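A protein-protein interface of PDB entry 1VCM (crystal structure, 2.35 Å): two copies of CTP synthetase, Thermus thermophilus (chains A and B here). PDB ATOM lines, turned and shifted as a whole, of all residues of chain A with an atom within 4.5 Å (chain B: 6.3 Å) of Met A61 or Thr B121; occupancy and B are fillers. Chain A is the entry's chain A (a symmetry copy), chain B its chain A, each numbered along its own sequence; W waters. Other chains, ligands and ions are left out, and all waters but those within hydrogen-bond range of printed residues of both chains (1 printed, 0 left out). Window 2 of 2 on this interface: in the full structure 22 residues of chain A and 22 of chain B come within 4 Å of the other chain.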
ATOM      1  N   TYR A  53     -21.802  26.228   0.077  1.00  0.00           N
ATOM      2  CA  TYR A  53     -21.132  25.315  -0.841  1.00  0.00           C
ATOM      3  C   TYR A  53     -19.757  25.807  -1.313  1.00  0.00           C
ATOM      4  O   TYR A  53     -19.415  26.975  -1.183  1.00  0.00           O
ATOM      5  CB  TYR A  53     -22.051  24.915  -2.012  1.00  0.00           C
ATOM      6  CG  TYR A  53     -22.656  26.013  -2.861  1.00  0.00           C
ATOM      7  CD1 TYR A  53     -21.852  26.958  -3.509  1.00  0.00           C
ATOM      8  CD2 TYR A  53     -24.034  26.041  -3.108  1.00  0.00           C
ATOM      9  CE1 TYR A  53     -22.408  27.896  -4.390  1.00  0.00           C
ATOM     10  CE2 TYR A  53     -24.596  26.975  -3.992  1.00  0.00           C
ATOM     11  CZ  TYR A  53     -23.775  27.895  -4.631  1.00  0.00           C
ATOM     12  OH  TYR A  53     -24.310  28.772  -5.545  1.00  0.00           O
ATOM     13  N   ASN A  55     -18.571  25.797  -4.423  1.00  0.00           N
ATOM     14  CA  ASN A  55     -18.592  26.452  -5.731  1.00  0.00           C
ATOM     15  C   ASN A  55     -18.328  27.947  -5.522  1.00  0.00           C
ATOM     16  O   ASN A  55     -18.892  28.561  -4.617  1.00  0.00           O
ATOM     17  CB  ASN A  55     -19.960  26.273  -6.403  1.00  0.00           C
ATOM     18  CG  ASN A  55     -20.316  24.814  -6.647  1.00  0.00           C
ATOM     19  OD1 ASN A  55     -20.249  24.324  -7.777  1.00  0.00           O
ATOM     20  ND2 ASN A  55     -20.692  24.112  -5.585  1.00  0.00           N
ATOM     21  N   ALA A  58     -22.391  30.130  -9.140  1.00  0.00           N
ATOM     22  CA  ALA A  58     -23.215  29.150  -9.844  1.00  0.00           C
ATOM     23  C   ALA A  58     -22.826  29.003 -11.316  1.00  0.00           C
ATOM     24  O   ALA A  58     -23.573  28.443 -12.110  1.00  0.00           O
ATOM     25  CB  ALA A  58     -24.684  29.534  -9.729  1.00  0.00           C
ATOM     26  N   GLY A  59     -21.645  29.495 -11.666  1.00  0.00           N
ATOM     27  CA  GLY A  59     -21.184  29.425 -13.038  1.00  0.00           C
ATOM     28  C   GLY A  59     -20.969  28.046 -13.640  1.00  0.00           C
ATOM     29  O   GLY A  59     -21.333  27.822 -14.787  1.00  0.00           O
ATOM     30  N   THR A  60     -20.379  27.118 -12.893  1.00  0.00           N
ATOM     31  CA  THR A  60     -20.129  25.782 -13.435  1.00  0.00           C
ATOM     32  C   THR A  60     -21.277  24.806 -13.218  1.00  0.00           C
ATOM     33  O   THR A  60     -21.130  23.610 -13.464  1.00  0.00           O
ATOM     34  CB  THR A  60     -18.844  25.158 -12.833  1.00  0.00           C
ATOM     35  OG1 THR A  60     -19.027  24.926 -11.427  1.00  0.00           O
ATOM     36  CG2 THR A  60     -17.656  26.091 -13.041  1.00  0.00           C
ATOM     37  N   MET A  61     -22.419  25.318 -12.770  1.00  0.00           N
ATOM     38  CA  MET A  61     -23.589  24.480 -12.513  1.00  0.00           C
ATOM     39  C   MET A  61     -24.584  24.495 -13.670  1.00  0.00           C
ATOM     40  O   MET A  61     -24.596  25.430 -14.475  1.00  0.00           O
ATOM     41  CB  MET A  61     -24.298  24.949 -11.243  1.00  0.00           C
ATOM     42  CG  MET A  61     -23.413  25.017 -10.018  1.00  0.00           C
ATOM     43  SD  MET A  61     -24.363  25.504  -8.567  1.00  0.00           S
ATOM     44  CE  MET A  61     -24.976  23.911  -8.039  1.00  0.00           C
ATOM     45  N   ARG A  62     -25.414  23.457 -13.746  1.00  0.00           N
ATOM     46  CA  ARG A  62     -26.425  23.355 -14.798  1.00  0.00           C
ATOM     47  C   ARG A  62     -27.360  24.554 -14.671  1.00  0.00           C
ATOM     48  O   ARG A  62     -28.063  24.696 -13.673  1.00  0.00           O
ATOM     49  CB  ARG A  62     -27.212  22.049 -14.655  1.00  0.00           C
ATOM     50  N   PRO A  63     -27.376  25.434 -15.689  1.00  0.00           N
ATOM     51  CA  PRO A  63     -28.203  26.648 -15.744  1.00  0.00           C
ATOM     52  C   PRO A  63     -29.717  26.501 -15.552  1.00  0.00           C
ATOM     53  O   PRO A  63     -30.384  27.462 -15.152  1.00  0.00           O
ATOM     54  CB  PRO A  63     -27.844  27.248 -17.103  1.00  0.00           C
ATOM     55  CG  PRO A  63     -27.429  26.050 -17.907  1.00  0.00           C
ATOM     56  CD  PRO A  63     -26.590  25.292 -16.924  1.00  0.00           C
ATOM     57  N   ARG A 470     -27.253  35.689 -21.039  1.00  0.00           N
ATOM     58  CA  ARG A 470     -26.545  34.494 -20.599  1.00  0.00           C
ATOM     59  C   ARG A 470     -26.583  33.504 -21.771  1.00  0.00           C
ATOM     60  O   ARG A 470     -27.368  32.563 -21.761  1.00  0.00           O
ATOM     61  CB  ARG A 470     -27.233  33.888 -19.365  1.00  0.00           C
ATOM     62  CG  ARG A 470     -26.609  32.602 -18.828  1.00  0.00           C
ATOM     63  CD  ARG A 470     -27.546  31.940 -17.811  1.00  0.00           C
ATOM     64  NE  ARG A 470     -27.120  30.597 -17.433  1.00  0.00           N
ATOM     65  CZ  ARG A 470     -25.984  30.325 -16.801  1.00  0.00           C
ATOM     66  NH1 ARG A 470     -25.162  31.309 -16.471  1.00  0.00           N
ATOM     67  NH2 ARG A 470     -25.658  29.072 -16.502  1.00  0.00           N
ATOM     68  N   GLU B 112     -13.390  22.459  -9.262  1.00  0.00           N
ATOM     69  CA  GLU B 112     -14.733  22.828  -9.690  1.00  0.00           C
ATOM     70  C   GLU B 112     -14.743  24.046 -10.609  1.00  0.00           C
ATOM     71  O   GLU B 112     -15.659  24.188 -11.409  1.00  0.00           O
ATOM     72  CB  GLU B 112     -15.681  23.009  -8.491  1.00  0.00           C
ATOM     73  CG  GLU B 112     -15.657  24.332  -7.789  1.00  0.00           C
ATOM     74  CD  GLU B 112     -16.548  25.373  -8.442  1.00  0.00           C
ATOM     75  OE1 GLU B 112     -17.675  25.045  -8.867  1.00  0.00           O
ATOM     76  OE2 GLU B 112     -16.124  26.534  -8.509  1.00  0.00           O
ATOM     77  N   TYR B 117     -16.107  18.818 -11.587  1.00  0.00           N
ATOM     78  CA  TYR B 117     -17.115  18.169 -10.767  1.00  0.00           C
ATOM     79  C   TYR B 117     -18.409  17.978 -11.549  1.00  0.00           C
ATOM     80  O   TYR B 117     -19.478  17.749 -10.979  1.00  0.00           O
ATOM     81  CB  TYR B 117     -17.346  18.944  -9.472  1.00  0.00           C
ATOM     82  CG  TYR B 117     -16.272  18.643  -8.452  1.00  0.00           C
ATOM     83  CD1 TYR B 117     -15.364  19.621  -8.052  1.00  0.00           C
ATOM     84  CD2 TYR B 117     -16.131  17.357  -7.921  1.00  0.00           C
ATOM     85  CE1 TYR B 117     -14.338  19.329  -7.151  1.00  0.00           C
ATOM     86  CE2 TYR B 117     -15.107  17.054  -7.022  1.00  0.00           C
ATOM     87  CZ  TYR B 117     -14.216  18.043  -6.644  1.00  0.00           C
ATOM     88  OH  TYR B 117     -13.200  17.756  -5.765  1.00  0.00           O
ATOM     89  N   SER B 119     -20.620  19.828 -13.038  1.00  0.00           N
ATOM     90  CA  SER B 119     -21.809  20.630 -12.755  1.00  0.00           C
ATOM     91  C   SER B 119     -22.573  20.379 -11.456  1.00  0.00           C
ATOM     92  O   SER B 119     -23.624  20.988 -11.242  1.00  0.00           O
ATOM     93  CB  SER B 119     -22.793  20.522 -13.929  1.00  0.00           C
ATOM     94  OG  SER B 119     -22.180  20.915 -15.142  1.00  0.00           O
ATOM     95  N   GLN B 120     -22.080  19.495 -10.597  1.00  0.00           N
ATOM     96  CA  GLN B 120     -22.769  19.238  -9.330  1.00  0.00           C
ATOM     97  C   GLN B 120     -22.429  20.390  -8.395  1.00  0.00           C
ATOM     98  O   GLN B 120     -21.491  21.146  -8.652  1.00  0.00           O
ATOM     99  CB  GLN B 120     -22.269  17.947  -8.674  1.00  0.00           C
ATOM    100  CG  GLN B 120     -21.851  16.842  -9.629  1.00  0.00           C
ATOM    101  CD  GLN B 120     -20.841  15.883  -9.003  1.00  0.00           C
ATOM    102  OE1 GLN B 120     -20.281  15.017  -9.683  1.00  0.00           O
ATOM    103  NE2 GLN B 120     -20.601  16.038  -7.704  1.00  0.00           N
ATOM    104  N   THR B 121     -23.195  20.532  -7.319  1.00  0.00           N
ATOM    105  CA  THR B 121     -22.903  21.557  -6.328  1.00  0.00           C
ATOM    106  C   THR B 121     -21.862  20.890  -5.426  1.00  0.00           C
ATOM    107  O   THR B 121     -22.060  19.769  -4.968  1.00  0.00           O
ATOM    108  CB  THR B 121     -24.164  21.953  -5.532  1.00  0.00           C
ATOM    109  OG1 THR B 121     -23.807  22.232  -4.172  1.00  0.00           O
ATOM    110  CG2 THR B 121     -25.192  20.858  -5.578  1.00  0.00           C
ATOM    111  N   VAL B 122     -20.745  21.569  -5.193  1.00  0.00           N
ATOM    112  CA  VAL B 122     -19.662  21.007  -4.395  1.00  0.00           C
ATOM    113  C   VAL B 122     -19.716  21.426  -2.929  1.00  0.00           C
ATOM    114  O   VAL B 122     -19.831  22.605  -2.610  1.00  0.00           O
ATOM    115  CB  VAL B 122     -18.300  21.390  -5.019  1.00  0.00           C
ATOM    116  CG1 VAL B 122     -17.179  20.606  -4.368  1.00  0.00           C
ATOM    117  CG2 VAL B 122     -18.335  21.113  -6.521  1.00  0.00           C
ATOM    118  N   GLN B 123     -19.599  20.446  -2.037  1.00  0.00           N
ATOM    119  CA  GLN B 123     -19.698  20.706  -0.607  1.00  0.00           C
ATOM    120  C   GLN B 123     -18.599  20.103   0.250  1.00  0.00           C
ATOM    121  O   GLN B 123     -17.920  19.167  -0.161  1.00  0.00           O
ATOM    122  CB  GLN B 123     -21.041  20.181  -0.104  1.00  0.00           C
ATOM    123  CG  GLN B 123     -22.247  20.825  -0.750  1.00  0.00           C
ATOM    124  CD  GLN B 123     -23.530  20.116  -0.379  1.00  0.00           C
ATOM    125  OE1 GLN B 123     -23.986  19.230  -1.094  1.00  0.00           O
ATOM    126  NE2 GLN B 123     -24.109  20.488   0.761  1.00  0.00           N
ATOM    127  N   HIS B 127     -17.203  16.191  -1.017  1.00  0.00           N
ATOM    128  CA  HIS B 127     -16.044  16.646  -1.779  1.00  0.00           C
ATOM    129  C   HIS B 127     -14.782  17.039  -1.035  1.00  0.00           C
ATOM    130  O   HIS B 127     -13.697  16.580  -1.389  1.00  0.00           O
ATOM    131  CB  HIS B 127     -16.477  17.756  -2.735  1.00  0.00           C
ATOM    132  CG  HIS B 127     -17.685  17.391  -3.538  1.00  0.00           C
ATOM    133  ND1 HIS B 127     -18.962  17.767  -3.174  1.00  0.00           N
ATOM    134  CD2 HIS B 127     -17.823  16.598  -4.627  1.00  0.00           C
ATOM    135  CE1 HIS B 127     -19.834  17.221  -4.002  1.00  0.00           C
ATOM    136  NE2 HIS B 127     -19.168  16.506  -4.894  1.00  0.00           N
HETATM  137  O   HOH W   1     -19.469  21.842 -10.547  1.00  0.00           O
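The backbone NH (N) of Val B122 sits close to the side-chain amide nitrogen (ND2) of Asn A55 (2.6 Å).
The side-chain carboxylate of Glu B112 lies close to the side-chain amide oxygen of Asn A55, 2.9 Å away.
The side-chain carboxylate of Glu B112 lies within hydrogen-bond range of the side-chain hydroxyl of Thr A60 (2.9 Å).
OG of Ser B119 sits close to O of Thr A60.
A ring nitrogen (NE2) of His B127 lies within hydrogen-bond range of the side-chain amide nitrogen of Gln B120 (3.2 Å).
The backbone carbonyl oxygen of Tyr B117 lies close to the side-chain amide oxygen of Gln B120 (3.1 Å).
Among the printed residues, merely in contact across the chains: Tyr A53 with Val B122 (3.3 Å), Met A61 with Thr B121 (3.3 Å), Asn A55 with Thr B121 (3.4 Å), Asn A55 with Gln B120 (3.5 Å), Met A61 with Ser B119 (3.7 Å), Tyr A53 with Thr B121 (3.9 Å) and Arg A62 with Ser B119 (3.9 Å).
Of chain A, only Tyr A53 (3.9 Å), Asn A55 (3.4 Å) and Met A61 (3.3 Å) come within 4 Å of Thr B121.
Printed residues of chain A within 4 Å of Val B122: Tyr A53 (3.3 Å) and Asn A55 (2.6 Å).
Of the printed residues of chain B, Asn A55 touches Glu B112 (2.9 Å), Gln B120 (3.5 Å), Thr B121 (3.4 Å) and Val B122 (2.6 Å).
Of the printed residues of chain B, Thr A60 touches Glu B112 (2.9 Å) and Ser B119 (3.1 Å).
Arg A470 touches none of the printed residues of chain B.
Gly A59 touches none of the printed residues of chain B.
The nearest printed residue of chain A that does not touch Thr B121 is Thr A60 (7.2 Å).
Of the 9 printed residues of chain A, 5 touch a printed residue of chain B.
Hydrophobic or aromatic side chains of chain A that line the printed part of chain B: Tyr A53 and Met A61.
Along chain A the printed residues that touch a printed residue of chain B span positions 53 to 62.
Hydrophobic or aromatic side chains of chain B that line the printed part of chain A: Val B122.
Among the printed residues, no Asp or Glu carboxylate lies within 4 Å of a Lys or Arg side-chain nitrogen of the other chain.
No position is printed for both chains.
Of the 11 pairs that touch across the chains among the printed residues, none has its exchanged pair printed and touching as well.
Water W1 lies within hydrogen-bond range of O of Gln B120, OG1 of Thr A60 and N of Ser B119.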
